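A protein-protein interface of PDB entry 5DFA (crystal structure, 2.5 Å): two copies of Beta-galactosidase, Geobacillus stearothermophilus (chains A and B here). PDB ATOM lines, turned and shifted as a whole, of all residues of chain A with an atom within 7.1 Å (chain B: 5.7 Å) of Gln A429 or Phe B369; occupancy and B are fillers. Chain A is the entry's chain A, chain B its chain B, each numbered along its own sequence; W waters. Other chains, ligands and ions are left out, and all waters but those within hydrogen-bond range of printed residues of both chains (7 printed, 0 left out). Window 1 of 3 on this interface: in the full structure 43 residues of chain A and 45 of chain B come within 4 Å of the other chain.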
ATOM      1  N   TRP A 191      23.712 -19.057  -5.288  1.00  0.00           N
ATOM      2  CA  TRP A 191      24.012 -19.968  -4.190  1.00  0.00           C
ATOM      3  C   TRP A 191      23.474 -19.452  -2.858  1.00  0.00           C
ATOM      4  O   TRP A 191      23.497 -20.173  -1.859  1.00  0.00           O
ATOM      5  CB  TRP A 191      25.520 -20.200  -4.082  1.00  0.00           C
ATOM      6  CG  TRP A 191      26.108 -20.930  -5.251  1.00  0.00           C
ATOM      7  CD1 TRP A 191      25.439 -21.420  -6.334  1.00  0.00           C
ATOM      8  CD2 TRP A 191      27.490 -21.251  -5.454  1.00  0.00           C
ATOM      9  NE1 TRP A 191      26.317 -22.027  -7.199  1.00  0.00           N
ATOM     10  CE2 TRP A 191      27.582 -21.937  -6.682  1.00  0.00           C
ATOM     11  CE3 TRP A 191      28.657 -21.025  -4.718  1.00  0.00           C
ATOM     12  CZ2 TRP A 191      28.795 -22.398  -7.189  1.00  0.00           C
ATOM     13  CZ3 TRP A 191      29.860 -21.484  -5.223  1.00  0.00           C
ATOM     14  CH2 TRP A 191      29.920 -22.163  -6.447  1.00  0.00           C
ATOM     15  N   TRP A 192      22.996 -18.208  -2.858  1.00  0.00           N
ATOM     16  CA  TRP A 192      22.464 -17.564  -1.656  1.00  0.00           C
ATOM     17  C   TRP A 192      23.514 -17.566  -0.545  1.00  0.00           C
ATOM     18  O   TRP A 192      23.245 -17.983   0.581  1.00  0.00           O
ATOM     19  CB  TRP A 192      21.180 -18.265  -1.195  1.00  0.00           C
ATOM     20  CG  TRP A 192      20.302 -17.441  -0.297  1.00  0.00           C
ATOM     21  CD1 TRP A 192      20.252 -17.483   1.066  1.00  0.00           C
ATOM     22  CD2 TRP A 192      19.337 -16.461  -0.703  1.00  0.00           C
ATOM     23  NE1 TRP A 192      19.320 -16.587   1.534  1.00  0.00           N
ATOM     24  CE2 TRP A 192      18.744 -15.948   0.468  1.00  0.00           C
ATOM     25  CE3 TRP A 192      18.919 -15.967  -1.943  1.00  0.00           C
ATOM     26  CZ2 TRP A 192      17.758 -14.964   0.437  1.00  0.00           C
ATOM     27  CZ3 TRP A 192      17.939 -14.989  -1.972  1.00  0.00           C
ATOM     28  CH2 TRP A 192      17.369 -14.499  -0.790  1.00  0.00           C
ATOM     29  N   PHE A 195      23.718 -16.298   3.416  1.00  0.00           N
ATOM     30  CA  PHE A 195      23.424 -17.174   4.542  1.00  0.00           C
ATOM     31  C   PHE A 195      24.715 -17.643   5.215  1.00  0.00           C
ATOM     32  O   PHE A 195      25.646 -18.084   4.541  1.00  0.00           O
ATOM     33  CB  PHE A 195      22.592 -18.368   4.066  1.00  0.00           C
ATOM     34  CG  PHE A 195      22.244 -19.346   5.150  1.00  0.00           C
ATOM     35  CD1 PHE A 195      21.245 -19.060   6.066  1.00  0.00           C
ATOM     36  CD2 PHE A 195      22.897 -20.564   5.238  1.00  0.00           C
ATOM     37  CE1 PHE A 195      20.916 -19.964   7.059  1.00  0.00           C
ATOM     38  CE2 PHE A 195      22.570 -21.472   6.224  1.00  0.00           C
ATOM     39  CZ  PHE A 195      21.579 -21.172   7.136  1.00  0.00           C
ATOM     40  N   TRP A 196      24.757 -17.530   6.541  1.00  0.00           N
ATOM     41  CA  TRP A 196      25.937 -17.874   7.342  1.00  0.00           C
ATOM     42  C   TRP A 196      27.200 -17.138   6.887  1.00  0.00           C
ATOM     43  O   TRP A 196      28.311 -17.649   7.038  1.00  0.00           O
ATOM     44  CB  TRP A 196      26.180 -19.390   7.325  1.00  0.00           C
ATOM     45  CG  TRP A 196      25.213 -20.168   8.175  1.00  0.00           C
ATOM     46  CD1 TRP A 196      24.264 -19.659   9.012  1.00  0.00           C
ATOM     47  CD2 TRP A 196      25.107 -21.596   8.270  1.00  0.00           C
ATOM     48  NE1 TRP A 196      23.571 -20.679   9.620  1.00  0.00           N
ATOM     49  CE2 TRP A 196      24.069 -21.878   9.180  1.00  0.00           C
ATOM     50  CE3 TRP A 196      25.784 -22.660   7.669  1.00  0.00           C
ATOM     51  CZ2 TRP A 196      23.693 -23.179   9.503  1.00  0.00           C
ATOM     52  CZ3 TRP A 196      25.410 -23.953   7.993  1.00  0.00           C
ATOM     53  CH2 TRP A 196      24.376 -24.201   8.903  1.00  0.00           C
ATOM     54  N   HIS A 215      30.354 -27.703   3.220  1.00  0.00           N
ATOM     55  CA  HIS A 215      29.431 -28.708   2.705  1.00  0.00           C
ATOM     56  C   HIS A 215      27.986 -28.319   2.992  1.00  0.00           C
ATOM     57  O   HIS A 215      27.086 -29.157   2.938  1.00  0.00           O
ATOM     58  CB  HIS A 215      29.739 -30.084   3.303  1.00  0.00           C
ATOM     59  CG  HIS A 215      29.837 -30.088   4.797  1.00  0.00           C
ATOM     60  ND1 HIS A 215      28.729 -30.053   5.618  1.00  0.00           N
ATOM     61  CD2 HIS A 215      30.912 -30.127   5.620  1.00  0.00           C
ATOM     62  CE1 HIS A 215      29.118 -30.067   6.880  1.00  0.00           C
ATOM     63  NE2 HIS A 215      30.439 -30.112   6.910  1.00  0.00           N
ATOM     64  N   THR A 216      27.769 -27.041   3.285  1.00  0.00           N
ATOM     65  CA  THR A 216      26.443 -26.559   3.648  1.00  0.00           C
ATOM     66  C   THR A 216      25.846 -25.627   2.593  1.00  0.00           C
ATOM     67  O   THR A 216      24.739 -25.117   2.767  1.00  0.00           O
ATOM     68  CB  THR A 216      26.465 -25.827   5.002  1.00  0.00           C
ATOM     69  OG1 THR A 216      27.289 -24.658   4.906  1.00  0.00           O
ATOM     70  CG2 THR A 216      27.009 -26.740   6.092  1.00  0.00           C
ATOM     71  N   ILE A 217      26.577 -25.405   1.506  1.00  0.00           N
ATOM     72  CA  ILE A 217      26.066 -24.595   0.406  1.00  0.00           C
ATOM     73  C   ILE A 217      25.618 -25.488  -0.747  1.00  0.00           C
ATOM     74  O   ILE A 217      26.446 -26.017  -1.491  1.00  0.00           O
ATOM     75  CB  ILE A 217      27.115 -23.587  -0.100  1.00  0.00           C
ATOM     76  CG1 ILE A 217      27.742 -22.833   1.074  1.00  0.00           C
ATOM     77  CG2 ILE A 217      26.488 -22.621  -1.095  1.00  0.00           C
ATOM     78  CD1 ILE A 217      28.733 -21.767   0.656  1.00  0.00           C
ATOM     79  N   HIS A 218      24.305 -25.647  -0.887  1.00  0.00           N
ATOM     80  CA  HIS A 218      23.729 -26.558  -1.874  1.00  0.00           C
ATOM     81  C   HIS A 218      24.105 -26.196  -3.308  1.00  0.00           C
ATOM     82  O   HIS A 218      24.397 -27.076  -4.118  1.00  0.00           O
ATOM     83  CB  HIS A 218      22.207 -26.588  -1.742  1.00  0.00           C
ATOM     84  CG  HIS A 218      21.724 -27.065  -0.407  1.00  0.00           C
ATOM     85  ND1 HIS A 218      22.195 -28.215   0.188  1.00  0.00           N
ATOM     86  CD2 HIS A 218      20.804 -26.550   0.442  1.00  0.00           C
ATOM     87  CE1 HIS A 218      21.591 -28.385   1.351  1.00  0.00           C
ATOM     88  NE2 HIS A 218      20.742 -27.389   1.528  1.00  0.00           N
ATOM     89  N   ASN A 221      27.523 -27.435  -3.956  1.00  0.00           N
ATOM     90  CA  ASN A 221      27.508 -28.889  -4.082  1.00  0.00           C
ATOM     91  C   ASN A 221      26.954 -29.333  -5.430  1.00  0.00           C
ATOM     92  O   ASN A 221      27.470 -30.264  -6.049  1.00  0.00           O
ATOM     93  CB  ASN A 221      26.689 -29.517  -2.953  1.00  0.00           C
ATOM     94  CG  ASN A 221      27.253 -29.207  -1.580  1.00  0.00           C
ATOM     95  OD1 ASN A 221      28.440 -28.917  -1.433  1.00  0.00           O
ATOM     96  ND2 ASN A 221      26.402 -29.273  -0.562  1.00  0.00           N
ATOM     97  N   ALA A 424      20.173 -32.624  -6.268  1.00  0.00           N
ATOM     98  CA  ALA A 424      19.682 -31.542  -5.420  1.00  0.00           C
ATOM     99  C   ALA A 424      18.735 -32.052  -4.338  1.00  0.00           C
ATOM    100  O   ALA A 424      18.789 -31.599  -3.194  1.00  0.00           O
ATOM    101  CB  ALA A 424      18.993 -30.483  -6.263  1.00  0.00           C
ATOM    102  N   LEU A 425      17.872 -32.993  -4.705  1.00  0.00           N
ATOM    103  CA  LEU A 425      16.908 -33.553  -3.766  1.00  0.00           C
ATOM    104  C   LEU A 425      17.606 -34.324  -2.649  1.00  0.00           C
ATOM    105  O   LEU A 425      17.221 -34.227  -1.484  1.00  0.00           O
ATOM    106  CB  LEU A 425      15.917 -34.464  -4.494  1.00  0.00           C
ATOM    107  CG  LEU A 425      14.852 -35.152  -3.639  1.00  0.00           C
ATOM    108  CD1 LEU A 425      14.064 -34.132  -2.833  1.00  0.00           C
ATOM    109  CD2 LEU A 425      13.926 -35.985  -4.511  1.00  0.00           C
ATOM    110  N   ASN A 426      18.634 -35.084  -3.010  1.00  0.00           N
ATOM    111  CA  ASN A 426      19.380 -35.872  -2.034  1.00  0.00           C
ATOM    112  C   ASN A 426      20.188 -35.006  -1.072  1.00  0.00           C
ATOM    113  O   ASN A 426      20.370 -35.363   0.090  1.00  0.00           O
ATOM    114  CB  ASN A 426      20.312 -36.856  -2.745  1.00  0.00           C
ATOM    115  CG  ASN A 426      19.628 -38.163  -3.090  1.00  0.00           C
ATOM    116  OD1 ASN A 426      18.562 -38.480  -2.560  1.00  0.00           O
ATOM    117  ND2 ASN A 426      20.241 -38.934  -3.979  1.00  0.00           N
ATOM    118  N   ASP A 427      20.667 -33.867  -1.561  1.00  0.00           N
ATOM    119  CA  ASP A 427      21.503 -32.981  -0.758  1.00  0.00           C
ATOM    120  C   ASP A 427      20.672 -32.049   0.121  1.00  0.00           C
ATOM    121  O   ASP A 427      21.191 -31.435   1.053  1.00  0.00           O
ATOM    122  CB  ASP A 427      22.424 -32.159  -1.663  1.00  0.00           C
ATOM    123  CG  ASP A 427      23.515 -31.445  -0.889  1.00  0.00           C
ATOM    124  OD1 ASP A 427      24.230 -32.114  -0.114  1.00  0.00           O
ATOM    125  OD2 ASP A 427      23.654 -30.213  -1.051  1.00  0.00           O
ATOM    126  N   ALA A 428      19.379 -31.953  -0.176  1.00  0.00           N
ATOM    127  CA  ALA A 428      18.500 -31.009   0.506  1.00  0.00           C
ATOM    128  C   ALA A 428      18.270 -31.366   1.973  1.00  0.00           C
ATOM    129  O   ALA A 428      18.058 -32.529   2.316  1.00  0.00           O
ATOM    130  CB  ALA A 428      17.165 -30.921  -0.222  1.00  0.00           C
ATOM    131  N   GLN A 429      18.319 -30.352   2.831  1.00  0.00           N
ATOM    132  CA  GLN A 429      17.972 -30.513   4.238  1.00  0.00           C
ATOM    133  C   GLN A 429      16.480 -30.287   4.431  1.00  0.00           C
ATOM    134  O   GLN A 429      16.011 -29.150   4.467  1.00  0.00           O
ATOM    135  CB  GLN A 429      18.771 -29.548   5.115  1.00  0.00           C
ATOM    136  CG  GLN A 429      20.264 -29.802   5.114  1.00  0.00           C
ATOM    137  CD  GLN A 429      20.645 -31.056   5.879  1.00  0.00           C
ATOM    138  OE1 GLN A 429      20.329 -31.197   7.061  1.00  0.00           O
ATOM    139  NE2 GLN A 429      21.330 -31.972   5.207  1.00  0.00           N
ATOM    140  N   GLY A 430      15.740 -31.382   4.549  1.00  0.00           N
ATOM    141  CA  GLY A 430      14.298 -31.324   4.688  1.00  0.00           C
ATOM    142  C   GLY A 430      13.703 -32.684   4.399  1.00  0.00           C
ATOM    143  O   GLY A 430      14.432 -33.622   4.070  1.00  0.00           O
ATOM    144  N   PHE A 431      12.382 -32.786   4.518  1.00  0.00           N
ATOM    145  CA  PHE A 431      11.676 -34.046   4.316  1.00  0.00           C
ATOM    146  C   PHE A 431      12.260 -35.125   5.227  1.00  0.00           C
ATOM    147  O   PHE A 431      12.545 -34.870   6.396  1.00  0.00           O
ATOM    148  CB  PHE A 431      11.746 -34.475   2.847  1.00  0.00           C
ATOM    149  CG  PHE A 431      11.573 -33.340   1.875  1.00  0.00           C
ATOM    150  CD1 PHE A 431      10.345 -32.717   1.726  1.00  0.00           C
ATOM    151  CD2 PHE A 431      12.642 -32.894   1.113  1.00  0.00           C
ATOM    152  CE1 PHE A 431      10.185 -31.671   0.834  1.00  0.00           C
ATOM    153  CE2 PHE A 431      12.488 -31.849   0.220  1.00  0.00           C
ATOM    154  CZ  PHE A 431      11.258 -31.237   0.080  1.00  0.00           C
ATOM    155  N   LYS A 436      13.131 -40.317   0.911  1.00  0.00           N
ATOM    156  CA  LYS A 436      13.126 -39.550  -0.334  1.00  0.00           C
ATOM    157  C   LYS A 436      12.945 -40.488  -1.518  1.00  0.00           C
ATOM    158  O   LYS A 436      11.955 -40.388  -2.245  1.00  0.00           O
ATOM    159  CB  LYS A 436      14.414 -38.739  -0.487  1.00  0.00           C
ATOM    160  CG  LYS A 436      14.524 -37.552   0.456  1.00  0.00           C
ATOM    161  CD  LYS A 436      15.868 -36.857   0.308  1.00  0.00           C
ATOM    162  CE  LYS A 436      16.002 -35.697   1.279  1.00  0.00           C
ATOM    163  NZ  LYS A 436      17.380 -35.134   1.279  1.00  0.00           N
ATOM    164  N   TYR A 477      11.358 -32.162  -7.992  1.00  0.00           N
ATOM    165  CA  TYR A 477      11.766 -31.156  -7.014  1.00  0.00           C
ATOM    166  C   TYR A 477      12.480 -29.973  -7.658  1.00  0.00           C
ATOM    167  O   TYR A 477      12.080 -28.822  -7.481  1.00  0.00           O
ATOM    168  CB  TYR A 477      12.655 -31.823  -5.958  1.00  0.00           C
ATOM    169  CG  TYR A 477      13.451 -30.891  -5.073  1.00  0.00           C
ATOM    170  CD1 TYR A 477      14.772 -30.583  -5.370  1.00  0.00           C
ATOM    171  CD2 TYR A 477      12.894 -30.348  -3.922  1.00  0.00           C
ATOM    172  CE1 TYR A 477      15.511 -29.744  -4.559  1.00  0.00           C
ATOM    173  CE2 TYR A 477      13.627 -29.508  -3.103  1.00  0.00           C
ATOM    174  CZ  TYR A 477      14.934 -29.210  -3.427  1.00  0.00           C
ATOM    175  OH  TYR A 477      15.670 -28.375  -2.619  1.00  0.00           O
ATOM    176  N   ASP A 510      19.057 -24.782  -7.215  1.00  0.00           N
ATOM    177  CA  ASP A 510      18.483 -25.203  -5.937  1.00  0.00           C
ATOM    178  C   ASP A 510      17.953 -23.998  -5.159  1.00  0.00           C
ATOM    179  O   ASP A 510      17.896 -24.008  -3.929  1.00  0.00           O
ATOM    180  CB  ASP A 510      19.498 -25.983  -5.095  1.00  0.00           C
ATOM    181  CG  ASP A 510      18.831 -26.854  -4.045  1.00  0.00           C
ATOM    182  OD1 ASP A 510      17.778 -27.454  -4.350  1.00  0.00           O
ATOM    183  OD2 ASP A 510      19.347 -26.935  -2.912  1.00  0.00           O
ATOM    184  N   ASN B 329      14.955 -28.331   9.707  1.00  0.00           N
ATOM    185  CA  ASN B 329      15.473 -28.847   8.447  1.00  0.00           C
ATOM    186  C   ASN B 329      16.430 -30.021   8.621  1.00  0.00           C
ATOM    187  O   ASN B 329      16.683 -30.767   7.676  1.00  0.00           O
ATOM    188  CB  ASN B 329      16.186 -27.733   7.679  1.00  0.00           C
ATOM    189  CG  ASN B 329      17.406 -27.210   8.415  1.00  0.00           C
ATOM    190  OD1 ASN B 329      17.331 -26.859   9.594  1.00  0.00           O
ATOM    191  ND2 ASN B 329      18.540 -27.168   7.725  1.00  0.00           N
ATOM    192  N   TRP B 330      16.951 -30.188   9.832  1.00  0.00           N
ATOM    193  CA  TRP B 330      18.097 -31.067  10.042  1.00  0.00           C
ATOM    194  C   TRP B 330      17.800 -32.353  10.818  1.00  0.00           C
ATOM    195  O   TRP B 330      18.714 -33.125  11.103  1.00  0.00           O
ATOM    196  CB  TRP B 330      19.206 -30.289  10.754  1.00  0.00           C
ATOM    197  CG  TRP B 330      18.770 -29.686  12.049  1.00  0.00           C
ATOM    198  CD1 TRP B 330      18.240 -28.443  12.239  1.00  0.00           C
ATOM    199  CD2 TRP B 330      18.821 -30.302  13.340  1.00  0.00           C
ATOM    200  NE1 TRP B 330      17.961 -28.246  13.569  1.00  0.00           N
ATOM    201  CE2 TRP B 330      18.308 -29.373  14.267  1.00  0.00           C
ATOM    202  CE3 TRP B 330      19.252 -31.548  13.803  1.00  0.00           C
ATOM    203  CZ2 TRP B 330      18.215 -29.652  15.629  1.00  0.00           C
ATOM    204  CZ3 TRP B 330      19.159 -31.821  15.153  1.00  0.00           C
ATOM    205  CH2 TRP B 330      18.645 -30.880  16.051  1.00  0.00           C
ATOM    206  N   ASN B 334      11.759 -34.488   9.270  1.00  0.00           N
ATOM    207  CA  ASN B 334      11.352 -33.111   9.521  1.00  0.00           C
ATOM    208  C   ASN B 334       9.844 -32.924   9.416  1.00  0.00           C
ATOM    209  O   ASN B 334       9.325 -32.482   8.391  1.00  0.00           O
ATOM    210  CB  ASN B 334      12.072 -32.165   8.562  1.00  0.00           C
ATOM    211  CG  ASN B 334      13.573 -32.155   8.777  1.00  0.00           C
ATOM    212  OD1 ASN B 334      14.066 -31.611   9.766  1.00  0.00           O
ATOM    213  ND2 ASN B 334      14.308 -32.761   7.853  1.00  0.00           N
ATOM    214  N   GLY B 367      17.825 -19.925  -0.198  1.00  0.00           N
ATOM    215  CA  GLY B 367      18.754 -20.978  -0.565  1.00  0.00           C
ATOM    216  C   GLY B 367      19.606 -21.462   0.590  1.00  0.00           C
ATOM    217  O   GLY B 367      19.390 -21.074   1.740  1.00  0.00           O
ATOM    218  N   SER B 368      20.567 -22.324   0.266  1.00  0.00           N
ATOM    219  CA  SER B 368      21.539 -22.870   1.215  1.00  0.00           C
ATOM    220  C   SER B 368      20.915 -23.805   2.256  1.00  0.00           C
ATOM    221  O   SER B 368      19.752 -24.197   2.146  1.00  0.00           O
ATOM    222  CB  SER B 368      22.299 -21.739   1.917  1.00  0.00           C
ATOM    223  OG  SER B 368      23.452 -22.234   2.576  1.00  0.00           O
ATOM    224  N   PHE B 369      21.709 -24.138   3.271  1.00  0.00           N
ATOM    225  CA  PHE B 369      21.456 -25.271   4.165  1.00  0.00           C
ATOM    226  C   PHE B 369      20.106 -25.271   4.884  1.00  0.00           C
ATOM    227  O   PHE B 369      19.512 -26.332   5.083  1.00  0.00           O
ATOM    228  CB  PHE B 369      22.574 -25.344   5.209  1.00  0.00           C
ATOM    229  CG  PHE B 369      22.850 -26.734   5.710  1.00  0.00           C
ATOM    230  CD1 PHE B 369      23.388 -27.692   4.867  1.00  0.00           C
ATOM    231  CD2 PHE B 369      22.593 -27.077   7.027  1.00  0.00           C
ATOM    232  CE1 PHE B 369      23.654 -28.969   5.323  1.00  0.00           C
ATOM    233  CE2 PHE B 369      22.856 -28.355   7.491  1.00  0.00           C
ATOM    234  CZ  PHE B 369      23.389 -29.301   6.636  1.00  0.00           C
ATOM    235  N   GLU B 370      19.624 -24.099   5.280  1.00  0.00           N
ATOM    236  CA  GLU B 370      18.401 -24.026   6.074  1.00  0.00           C
ATOM    237  C   GLU B 370      17.256 -23.341   5.338  1.00  0.00           C
ATOM    238  O   GLU B 370      16.451 -22.638   5.950  1.00  0.00           O
ATOM    239  CB  GLU B 370      18.674 -23.302   7.394  1.00  0.00           C
ATOM    240  CG  GLU B 370      19.566 -24.081   8.345  1.00  0.00           C
ATOM    241  CD  GLU B 370      19.843 -23.333   9.631  1.00  0.00           C
ATOM    242  OE1 GLU B 370      19.729 -22.091   9.629  1.00  0.00           O
ATOM    243  OE2 GLU B 370      20.174 -23.985  10.643  1.00  0.00           O
ATOM    244  N   LYS B 371      17.172 -23.562   4.031  1.00  0.00           N
ATOM    245  CA  LYS B 371      16.137 -22.924   3.224  1.00  0.00           C
ATOM    246  C   LYS B 371      14.768 -23.563   3.448  1.00  0.00           C
ATOM    247  O   LYS B 371      13.743 -23.004   3.058  1.00  0.00           O
ATOM    248  CB  LYS B 371      16.504 -22.974   1.739  1.00  0.00           C
ATOM    249  CG  LYS B 371      16.422 -24.351   1.101  1.00  0.00           C
ATOM    250  CD  LYS B 371      16.763 -24.271  -0.382  1.00  0.00           C
ATOM    251  CE  LYS B 371      16.487 -25.582  -1.098  1.00  0.00           C
ATOM    252  NZ  LYS B 371      17.369 -26.682  -0.623  1.00  0.00           N
ATOM    253  N   PHE B 372      14.754 -24.734   4.078  1.00  0.00           N
ATOM    254  CA  PHE B 372      13.502 -25.423   4.369  1.00  0.00           C
ATOM    255  C   PHE B 372      13.223 -25.470   5.868  1.00  0.00           C
ATOM    256  O   PHE B 372      12.277 -26.122   6.313  1.00  0.00           O
ATOM    257  CB  PHE B 372      13.522 -26.837   3.784  1.00  0.00           C
ATOM    258  CG  PHE B 372      13.424 -26.868   2.285  1.00  0.00           C
ATOM    259  CD1 PHE B 372      12.682 -25.915   1.608  1.00  0.00           C
ATOM    260  CD2 PHE B 372      14.078 -27.846   1.553  1.00  0.00           C
ATOM    261  CE1 PHE B 372      12.588 -25.937   0.230  1.00  0.00           C
ATOM    262  CE2 PHE B 372      13.989 -27.872   0.173  1.00  0.00           C
ATOM    263  CZ  PHE B 372      13.243 -26.917  -0.489  1.00  0.00           C
ATOM    264  N   HIS B 373      14.053 -24.777   6.642  1.00  0.00           N
ATOM    265  CA  HIS B 373      13.805 -24.623   8.070  1.00  0.00           C
ATOM    266  C   HIS B 373      12.581 -23.738   8.264  1.00  0.00           C
ATOM    267  O   HIS B 373      12.365 -22.793   7.504  1.00  0.00           O
ATOM    268  CB  HIS B 373      15.024 -24.024   8.778  1.00  0.00           C
ATOM    269  CG  HIS B 373      14.945 -24.081  10.272  1.00  0.00           C
ATOM    270  ND1 HIS B 373      14.114 -23.262  11.007  1.00  0.00           N
ATOM    271  CD2 HIS B 373      15.597 -24.857  11.171  1.00  0.00           C
ATOM    272  CE1 HIS B 373      14.255 -23.534  12.292  1.00  0.00           C
ATOM    273  NE2 HIS B 373      15.150 -24.497  12.418  1.00  0.00           N
HETATM  274  O   HOH W   1      19.927 -23.961  -1.956  1.00  0.00           O
HETATM  275  O   HOH W   2      25.577 -19.873   2.649  1.00  0.00           O
HETATM  276  O   HOH W   3      17.037 -26.640   4.302  1.00  0.00           O
HETATM  277  O   HOH W   4      21.274 -19.936  11.018  1.00  0.00           O
HETATM  278  O   HOH W   5      25.839 -22.692   4.178  1.00  0.00           O
HETATM  279  O   HOH W   6      18.086 -27.676   1.725  1.00  0.00           O
HETATM  280  O   HOH W   7      22.871 -22.774  -2.023  1.00  0.00           O
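The backbone NH of Asn B334 lies within hydrogen-bond range of the backbone carbonyl oxygen of Phe A431 (3.0 Å).
The backbone carbonyl oxygen of Thr A216 sits at hydrogen-bond distance from the side-chain hydroxyl of Ser B368.
The backbone carbonyl oxygen of Thr A216 is in hydrogen-bond range of the backbone NH of Phe B369 (3.2 Å).
O of Asn B329 lies within hydrogen-bond range of N of Gly A430 (3.3 Å).
The side-chain carboxylate (OD2) of Asp A510 lies within salt-bridge range of the side-chain amino group (NZ) of Lys B371, 3.0 Å away.
The side-chain hydroxyl (OH) of Tyr A477 lies within hydrogen-bond range of the side-chain amino group (NZ) of Lys B371.
NE2 of His A218 lies close to O of Ser B368, 3.4 Å away.
The backbone NH (N) of Trp B330 sits at hydrogen-bond distance from the side-chain amide oxygen (OD1) of Asn B334 (3.2 Å).
The side-chain amide nitrogen (ND2) of Asn B329 is in hydrogen-bond range of the backbone carbonyl oxygen (O) of Phe B369, at 2.9 Å.
O of Asn B329 sits at hydrogen-bond distance from ND2 of Asn B334.
The side-chain carboxylate (OD2) of Asp A427 lies within hydrogen-bond range of a ring nitrogen (ND1) of His A218, 2.8 Å away.
The side-chain carboxylate (OD1) of Asp A510 sits at hydrogen-bond distance from the side-chain hydroxyl (OH) of Tyr A477, at 2.9 Å.
CD2 of Phe A195 touches OG of Ser B368, at 3.2 Å.
Glu B370 touches Phe A195 (OE1 to CZ, 3.2 Å).
Trp A196 touches Phe B369.
Glu B370 touches Trp A196 (OE2 to CZ2, 3.8 Å).
His A218 touches Phe B369.
Gln A429 touches Asn B329 (C to O, 3.3 Å).
Gln A429 touches Trp B330.
Phe B369 touches Gln A429 (O to CB, 3.3 Å).
Asn B334 touches Gly A430 (ND2 to CA, 3.5 Å).
Tyr A477 touches Phe B372 (OH to CE2, 3.3 Å).
Of chain B, only Asn B329, Trp B330, Phe B369 and Phe B372 come within 4 Å of Gln A429.
Printed residues of chain A within 4 Å of Phe B369: Trp A196 (3.9 Å), Thr A216 (3.2 Å), His A218 (3.5 Å) and Gln A429 (3.3 Å).
Printed residues of chain A within 4 Å of Trp B330: Gln A429.
Printed residues of chain B within 4 Å of Tyr A477: Lys B371 (3.1 Å) and Phe B372 (3.3 Å).
Of the printed residues of chain B, His A218 touches Ser B368 (3.1 Å), Phe B369 (3.5 Å) and Lys B371 (3.6 Å).
Of the printed residues of chain B, Phe A431 touches Asn B334 (3.0 Å).
The nearest residue of chain B that does not touch Gln A429 is Asn B334 (4.7 Å).
The nearest printed residue of chain A that does not touch Phe B372 is Phe A431 (4.3 Å).
Printed residues of chain A that touch a printed residue of chain B: Trp A192, Phe A195, Trp A196, Thr A216, His A218, Gln A429, Gly A430, Phe A431, Tyr A477 and Asp A510.
Hydrophobic or aromatic side chains of chain A that line the printed part of chain B: Trp A192, Phe A195, Trp A196, His A218 and Tyr A477.
Printed residues of chain B that touch a printed residue of chain A: Asn B329, Trp B330, Asn B334, Gly B367, Ser B368, Phe B369, Glu B370, Lys B371 and Phe B372.
Among the printed residues, 20 pairs touch across the chains.
No position is printed for both chains.
Water W2 bridges O of Phe A195 (2.6 Å) and OG of Ser B368 (3.2 Å).
Water W3 lies within hydrogen-bond range of O of Phe B369 (2.6 Å), O of Gln A429 (2.7 Å), N of Phe B372 (3.0 Å) and N of Lys B371 (3.1 Å).
Water W6 lies within hydrogen-bond range of NZ of Lys B371 (2.6 Å), NE2 of His A218 (2.7 Å) and N of Gln A429 (2.9 Å).
Water W7 lies within hydrogen-bond range of the backbone carbonyl oxygen (O) of Trp A191, the backbone NH (N) of Ser B368 and the backbone NH (N) of His A218.
Water W4 lies within hydrogen-bond range of NE1 of Trp A196 (2.8 Å) and OE1 of Glu B370 (3.0 Å).
Water W1 bridges O of Asp A510 (2.8 Å) and N of Ser B368 (2.8 Å).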
